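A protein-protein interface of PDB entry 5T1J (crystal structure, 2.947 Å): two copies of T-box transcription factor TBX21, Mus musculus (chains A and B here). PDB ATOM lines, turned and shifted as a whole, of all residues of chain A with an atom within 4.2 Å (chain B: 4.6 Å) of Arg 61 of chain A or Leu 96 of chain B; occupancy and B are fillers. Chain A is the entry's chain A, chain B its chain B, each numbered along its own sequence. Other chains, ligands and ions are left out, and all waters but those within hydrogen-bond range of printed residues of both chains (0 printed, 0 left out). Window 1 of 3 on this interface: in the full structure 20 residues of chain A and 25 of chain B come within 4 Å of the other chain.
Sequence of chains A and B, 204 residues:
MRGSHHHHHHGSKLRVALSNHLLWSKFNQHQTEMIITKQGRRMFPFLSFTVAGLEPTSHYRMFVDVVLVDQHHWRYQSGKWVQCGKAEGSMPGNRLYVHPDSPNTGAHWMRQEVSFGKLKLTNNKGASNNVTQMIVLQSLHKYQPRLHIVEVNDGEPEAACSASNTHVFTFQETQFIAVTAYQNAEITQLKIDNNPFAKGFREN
The guanidinium group (NH2) of Arg 61 of chain A is in hydrogen-bond range of the backbone carbonyl oxygen (O) of Asn 94 of chain B, at 3.2 Å.
The backbone carbonyl oxygen (O) of Ser 102 of chain A lies within hydrogen-bond range of the guanidinium group (NH1) of Arg 95 of chain B, at 3.0 Å.
The backbone NH (N) of Arg 61 of chain A is in hydrogen-bond range of the backbone carbonyl oxygen (O) of Val 150 of chain A (2.5 Å).
OG of Ser 102 of chain A sits at hydrogen-bond distance from N of Met 62 of chain A, 3.4 Å away.
The side-chain carboxylate of Asp 65 of chain B sits close to the side-chain amide nitrogen of Asn 94 of chain B (2.9 Å).
Arg 61 of chain A touches Arg 95 of chain B.
Leu 96 of chain B touches Arg 61 of chain A (CD1 to CZ, 3.3 Å).
Arg 61 of chain A touches just these residues of chain B: Asn 94 (3.2 Å), Arg 95 (3.4 Å) and Leu 96 (3.3 Å).
Leu 96 of chain B touches one residue of chain A.
Of the printed residues of chain A, Arg 95 of chain B touches Arg 61 and Ser 102.
Printed residues of chain B within 4 Å of Ser 102 of chain A: Arg 95.
Printed residues of chain A within 4 Å of Asn 94 of chain B: Arg 61 (3.2 Å).
The nearest printed residue of chain B that does not touch Arg 61 of chain A is Asp 65 of chain B (5.0 Å).
Hydrophobic or aromatic side chains of chain B that line the printed part of chain A: Leu 96.
Among the printed residues, no Asp or Glu carboxylate lies within 4 Å of a Lys or Arg side-chain nitrogen of the other chain.
Positions printed for both chains: 63, 96 and 98.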
ATOM      1  N   TYR A  60     -19.519 -12.703  10.533  1.00  0.00           N
ATOM      2  CA  TYR A  60     -19.830 -12.146   9.207  1.00  0.00           C
ATOM      3  C   TYR A  60     -21.305 -11.711   9.001  1.00  0.00           C
ATOM      4  O   TYR A  60     -22.207 -12.203   9.686  1.00  0.00           O
ATOM      5  CB  TYR A  60     -19.474 -13.180   8.145  1.00  0.00           C
ATOM      6  CG  TYR A  60     -18.196 -14.000   8.351  1.00  0.00           C
ATOM      7  CD1 TYR A  60     -17.032 -13.694   7.669  1.00  0.00           C
ATOM      8  CD2 TYR A  60     -18.188 -15.131   9.159  1.00  0.00           C
ATOM      9  CE1 TYR A  60     -15.891 -14.452   7.810  1.00  0.00           C
ATOM     10  CE2 TYR A  60     -17.042 -15.892   9.314  1.00  0.00           C
ATOM     11  CZ  TYR A  60     -15.897 -15.549   8.634  1.00  0.00           C
ATOM     12  OH  TYR A  60     -14.760 -16.309   8.787  1.00  0.00           O
ATOM     13  N   ARG A  61     -21.540 -10.810   8.042  1.00  0.00           N
ATOM     14  CA  ARG A  61     -22.899 -10.352   7.711  1.00  0.00           C
ATOM     15  C   ARG A  61     -23.537 -11.157   6.560  1.00  0.00           C
ATOM     16  O   ARG A  61     -22.933 -11.334   5.489  1.00  0.00           O
ATOM     17  CB  ARG A  61     -22.924  -8.860   7.350  1.00  0.00           C
ATOM     18  CG  ARG A  61     -23.883  -8.140   8.267  1.00  0.00           C
ATOM     19  CD  ARG A  61     -24.008  -6.597   8.121  1.00  0.00           C
ATOM     20  NE  ARG A  61     -24.695  -5.991   9.295  1.00  0.00           N
ATOM     21  CZ  ARG A  61     -25.865  -6.397   9.801  1.00  0.00           C
ATOM     22  NH1 ARG A  61     -26.540  -7.397   9.252  1.00  0.00           N
ATOM     23  NH2 ARG A  61     -26.389  -5.788  10.842  1.00  0.00           N
ATOM     24  N   MET A  62     -24.747 -11.670   6.783  1.00  0.00           N
ATOM     25  CA  MET A  62     -25.462 -12.333   5.697  1.00  0.00           C
ATOM     26  C   MET A  62     -26.874 -11.801   5.488  1.00  0.00           C
ATOM     27  O   MET A  62     -27.825 -12.105   6.232  1.00  0.00           O
ATOM     28  CB  MET A  62     -25.473 -13.834   5.948  1.00  0.00           C
ATOM     29  CG  MET A  62     -24.317 -14.531   5.259  1.00  0.00           C
ATOM     30  SD  MET A  62     -24.041 -16.186   5.899  1.00  0.00           S
ATOM     31  CE  MET A  62     -22.743 -16.775   4.800  1.00  0.00           C
ATOM     32  N   PHE A  63     -26.981 -11.018   4.427  1.00  0.00           N
ATOM     33  CA  PHE A  63     -28.238 -10.489   3.981  1.00  0.00           C
ATOM     34  C   PHE A  63     -28.366 -10.807   2.497  1.00  0.00           C
ATOM     35  O   PHE A  63     -27.359 -11.023   1.797  1.00  0.00           O
ATOM     36  CB  PHE A  63     -28.323  -8.984   4.208  1.00  0.00           C
ATOM     37  CG  PHE A  63     -27.412  -8.168   3.310  1.00  0.00           C
ATOM     38  CD1 PHE A  63     -27.930  -7.262   2.398  1.00  0.00           C
ATOM     39  CD2 PHE A  63     -26.025  -8.274   3.418  1.00  0.00           C
ATOM     40  CE1 PHE A  63     -27.082  -6.496   1.591  1.00  0.00           C
ATOM     41  CE2 PHE A  63     -25.179  -7.504   2.611  1.00  0.00           C
ATOM     42  CZ  PHE A  63     -25.719  -6.608   1.698  1.00  0.00           C
ATOM     43  N   LEU A  96     -33.163  -4.732   0.835  1.00  0.00           N
ATOM     44  CA  LEU A  96     -32.339  -5.718   1.488  1.00  0.00           C
ATOM     45  C   LEU A  96     -33.173  -6.615   2.410  1.00  0.00           C
ATOM     46  O   LEU A  96     -34.230  -6.206   2.908  1.00  0.00           O
ATOM     47  CB  LEU A  96     -31.188  -5.045   2.219  1.00  0.00           C
ATOM     48  CG  LEU A  96     -29.978  -4.736   1.328  1.00  0.00           C
ATOM     49  CD1 LEU A  96     -30.312  -3.989   0.065  1.00  0.00           C
ATOM     50  CD2 LEU A  96     -28.960  -3.953   2.104  1.00  0.00           C
ATOM     51  N   VAL A  98     -31.723  -8.975   5.530  1.00  0.00           N
ATOM     52  CA  VAL A  98     -30.764  -9.562   6.458  1.00  0.00           C
ATOM     53  C   VAL A  98     -31.358 -10.738   7.232  1.00  0.00           C
ATOM     54  O   VAL A  98     -32.460 -10.627   7.787  1.00  0.00           O
ATOM     55  CB  VAL A  98     -30.230  -8.448   7.508  1.00  0.00           C
ATOM     56  CG1 VAL A  98     -31.354  -7.574   8.019  1.00  0.00           C
ATOM     57  CG2 VAL A  98     -29.469  -9.041   8.719  1.00  0.00           C
ATOM     58  N   SER A 102     -28.531 -12.851  11.999  1.00  0.00           N
ATOM     59  CA  SER A 102     -27.290 -12.139  11.636  1.00  0.00           C
ATOM     60  C   SER A 102     -27.143 -10.841  12.430  1.00  0.00           C
ATOM     61  O   SER A 102     -28.125 -10.120  12.616  1.00  0.00           O
ATOM     62  CB  SER A 102     -27.267 -11.818  10.135  1.00  0.00           C
ATOM     63  OG  SER A 102     -26.229 -10.904   9.784  1.00  0.00           O
ATOM     64  N   HIS A 148     -24.780 -11.445  -0.157  1.00  0.00           N
ATOM     65  CA  HIS A 148     -23.453 -10.952   0.160  1.00  0.00           C
ATOM     66  C   HIS A 148     -23.031 -11.405   1.509  1.00  0.00           C
ATOM     67  O   HIS A 148     -23.850 -11.631   2.404  1.00  0.00           O
ATOM     68  CB  HIS A 148     -23.444  -9.445   0.139  1.00  0.00           C
ATOM     69  CG  HIS A 148     -24.584  -8.885  -0.632  1.00  0.00           C
ATOM     70  ND1 HIS A 148     -25.871  -8.919  -0.147  1.00  0.00           N
ATOM     71  CD2 HIS A 148     -24.652  -8.322  -1.858  1.00  0.00           C
ATOM     72  CE1 HIS A 148     -26.684  -8.378  -1.034  1.00  0.00           C
ATOM     73  NE2 HIS A 148     -25.970  -8.006  -2.082  1.00  0.00           N
ATOM     74  N   ILE A 149     -21.723 -11.463   1.667  1.00  0.00           N
ATOM     75  CA  ILE A 149     -21.165 -11.742   2.955  1.00  0.00           C
ATOM     76  C   ILE A 149     -20.081 -10.708   3.234  1.00  0.00           C
ATOM     77  O   ILE A 149     -18.936 -10.804   2.779  1.00  0.00           O
ATOM     78  CB  ILE A 149     -20.658 -13.196   3.044  1.00  0.00           C
ATOM     79  CG1 ILE A 149     -19.671 -13.540   1.928  1.00  0.00           C
ATOM     80  CG2 ILE A 149     -21.809 -14.136   2.910  1.00  0.00           C
ATOM     81  CD1 ILE A 149     -19.005 -14.893   2.131  1.00  0.00           C
ATOM     82  N   VAL A 150     -20.517  -9.665   3.936  1.00  0.00           N
ATOM     83  CA  VAL A 150     -19.641  -8.645   4.459  1.00  0.00           C
ATOM     84  C   VAL A 150     -19.143  -9.170   5.787  1.00  0.00           C
ATOM     85  O   VAL A 150     -19.951  -9.528   6.645  1.00  0.00           O
ATOM     86  CB  VAL A 150     -20.389  -7.312   4.632  1.00  0.00           C
ATOM     87  CG1 VAL A 150     -19.518  -6.275   5.308  1.00  0.00           C
ATOM     88  CG2 VAL A 150     -20.880  -6.803   3.287  1.00  0.00           C
ATOM     89  N   PHE B  63     -28.709   3.292   3.375  1.00  0.00           N
ATOM     90  CA  PHE B  63     -29.018   2.673   4.641  1.00  0.00           C
ATOM     91  C   PHE B  63     -27.952   3.051   5.681  1.00  0.00           C
ATOM     92  O   PHE B  63     -26.813   3.409   5.334  1.00  0.00           O
ATOM     93  CB  PHE B  63     -29.090   1.167   4.478  1.00  0.00           C
ATOM     94  CG  PHE B  63     -27.761   0.524   4.195  1.00  0.00           C
ATOM     95  CD1 PHE B  63     -27.171  -0.316   5.117  1.00  0.00           C
ATOM     96  CD2 PHE B  63     -27.084   0.780   3.004  1.00  0.00           C
ATOM     97  CE1 PHE B  63     -25.945  -0.931   4.849  1.00  0.00           C
ATOM     98  CE2 PHE B  63     -25.851   0.170   2.737  1.00  0.00           C
ATOM     99  CZ  PHE B  63     -25.290  -0.690   3.661  1.00  0.00           C
ATOM    100  N   VAL B  64     -28.278   2.895   6.954  1.00  0.00           N
ATOM    101  CA  VAL B  64     -27.285   3.239   7.933  1.00  0.00           C
ATOM    102  C   VAL B  64     -27.143   1.997   8.764  1.00  0.00           C
ATOM    103  O   VAL B  64     -28.086   1.202   8.850  1.00  0.00           O
ATOM    104  CB  VAL B  64     -27.694   4.469   8.831  1.00  0.00           C
ATOM    105  CG1 VAL B  64     -28.432   4.011  10.093  1.00  0.00           C
ATOM    106  CG2 VAL B  64     -26.504   5.231   9.251  1.00  0.00           C
ATOM    107  N   ASP B  65     -25.939   1.757   9.255  1.00  0.00           N
ATOM    108  CA  ASP B  65     -25.720   0.698  10.201  1.00  0.00           C
ATOM    109  C   ASP B  65     -24.874   1.267  11.346  1.00  0.00           C
ATOM    110  O   ASP B  65     -23.908   2.023  11.139  1.00  0.00           O
ATOM    111  CB  ASP B  65     -25.098  -0.506   9.532  1.00  0.00           C
ATOM    112  CG  ASP B  65     -23.632  -0.331   9.262  1.00  0.00           C
ATOM    113  OD1 ASP B  65     -23.237   0.801   8.927  1.00  0.00           O
ATOM    114  OD2 ASP B  65     -22.866  -1.306   9.412  1.00  0.00           O
ATOM    115  N   ASN B  94     -25.988  -4.064  15.789  1.00  0.00           N
ATOM    116  CA  ASN B  94     -26.394  -3.632  14.436  1.00  0.00           C
ATOM    117  C   ASN B  94     -27.438  -4.521  13.753  1.00  0.00           C
ATOM    118  O   ASN B  94     -27.432  -5.765  13.829  1.00  0.00           O
ATOM    119  CB  ASN B  94     -25.202  -3.476  13.493  1.00  0.00           C
ATOM    120  CG  ASN B  94     -25.529  -2.677  12.263  1.00  0.00           C
ATOM    121  OD1 ASN B  94     -26.648  -2.187  12.072  1.00  0.00           O
ATOM    122  ND2 ASN B  94     -24.566  -2.622  11.369  1.00  0.00           N
ATOM    123  N   ARG B  95     -28.328  -3.846  13.054  1.00  0.00           N
ATOM    124  CA  ARG B  95     -29.227  -4.484  12.120  1.00  0.00           C
ATOM    125  C   ARG B  95     -29.612  -3.266  11.356  1.00  0.00           C
ATOM    126  O   ARG B  95     -29.872  -2.212  11.962  1.00  0.00           O
ATOM    127  CB  ARG B  95     -30.402  -5.186  12.762  1.00  0.00           C
ATOM    128  CG  ARG B  95     -31.383  -5.803  11.747  1.00  0.00           C
ATOM    129  CD  ARG B  95     -32.579  -6.387  12.513  1.00  0.00           C
ATOM    130  NE  ARG B  95     -32.137  -7.021  13.773  1.00  0.00           N
ATOM    131  CZ  ARG B  95     -31.220  -7.990  13.895  1.00  0.00           C
ATOM    132  NH1 ARG B  95     -30.675  -8.557  12.824  1.00  0.00           N
ATOM    133  NH2 ARG B  95     -30.876  -8.447  15.099  1.00  0.00           N
ATOM    134  N   LEU B  96     -29.491  -3.361  10.043  1.00  0.00           N
ATOM    135  CA  LEU B  96     -29.517  -2.173   9.211  1.00  0.00           C
ATOM    136  C   LEU B  96     -30.768  -1.300   9.329  1.00  0.00           C
ATOM    137  O   LEU B  96     -31.790  -1.741   9.861  1.00  0.00           O
ATOM    138  CB  LEU B  96     -29.306  -2.601   7.775  1.00  0.00           C
ATOM    139  CG  LEU B  96     -27.852  -2.845   7.370  1.00  0.00           C
ATOM    140  CD1 LEU B  96     -27.065  -3.774   8.292  1.00  0.00           C
ATOM    141  CD2 LEU B  96     -27.908  -3.430   5.971  1.00  0.00           C
ATOM    142  N   TYR B  97     -30.653  -0.038   8.923  1.00  0.00           N
ATOM    143  CA  TYR B  97     -31.848   0.731   8.632  1.00  0.00           C
ATOM    144  C   TYR B  97     -31.688   1.546   7.354  1.00  0.00           C
ATOM    145  O   TYR B  97     -31.083   2.660   7.402  1.00  0.00           O
ATOM    146  CB  TYR B  97     -32.198   1.643   9.751  1.00  0.00           C
ATOM    147  CG  TYR B  97     -33.568   2.248   9.644  1.00  0.00           C
ATOM    148  CD1 TYR B  97     -34.637   1.686  10.326  1.00  0.00           C
ATOM    149  CD2 TYR B  97     -33.792   3.409   8.893  1.00  0.00           C
ATOM    150  CE1 TYR B  97     -35.897   2.252  10.264  1.00  0.00           C
ATOM    151  CE2 TYR B  97     -35.041   3.980   8.825  1.00  0.00           C
ATOM    152  CZ  TYR B  97     -36.096   3.398   9.508  1.00  0.00           C
ATOM    153  OH  TYR B  97     -37.352   3.953   9.447  1.00  0.00           O
ATOM    154  N   VAL B  98     -32.288   0.981   6.271  1.00  0.00           N
ATOM    155  CA  VAL B  98     -32.413   1.549   4.935  1.00  0.00           C
ATOM    156  C   VAL B  98     -33.512   2.597   4.880  1.00  0.00           C
ATOM    157  O   VAL B  98     -34.627   2.356   5.353  1.00  0.00           O
ATOM    158  CB  VAL B  98     -32.739   0.424   3.910  1.00  0.00           C
ATOM    159  CG1 VAL B  98     -33.846  -0.476   4.447  1.00  0.00           C
ATOM    160  CG2 VAL B  98     -33.153   0.970   2.529  1.00  0.00           C
ATOM    161  N   GLN B 133     -37.452  -3.978  11.173  1.00  0.00           N
ATOM    162  CA  GLN B 133     -36.496  -3.071  10.517  1.00  0.00           C
ATOM    163  C   GLN B 133     -36.063  -2.008  11.527  1.00  0.00           C
ATOM    164  O   GLN B 133     -36.124  -0.783  11.303  1.00  0.00           O
ATOM    165  CB  GLN B 133     -37.063  -2.434   9.250  1.00  0.00           C
ATOM    166  CG  GLN B 133     -36.029  -1.631   8.434  1.00  0.00           C
ATOM    167  CD  GLN B 133     -36.616  -1.039   7.159  1.00  0.00           C
ATOM    168  OE1 GLN B 133     -37.575  -1.589   6.582  1.00  0.00           O
ATOM    169  NE2 GLN B 133     -36.051   0.099   6.715  1.00  0.00           N
ATOM    170  N   ILE B 135     -32.942  -1.363  14.640  1.00  0.00           N
ATOM    171  CA  ILE B 135     -31.674  -1.784  15.191  1.00  0.00           C
ATOM    172  C   ILE B 135     -31.912  -2.329  16.561  1.00  0.00           C
ATOM    173  O   ILE B 135     -32.672  -1.761  17.340  1.00  0.00           O
ATOM    174  CB  ILE B 135     -30.674  -0.663  15.219  1.00  0.00           C
ATOM    175  CG1 ILE B 135     -30.736   0.057  13.877  1.00  0.00           C
ATOM    176  CG2 ILE B 135     -29.337  -1.239  15.403  1.00  0.00           C
ATOM    177  CD1 ILE B 135     -29.536   0.810  13.498  1.00  0.00           C
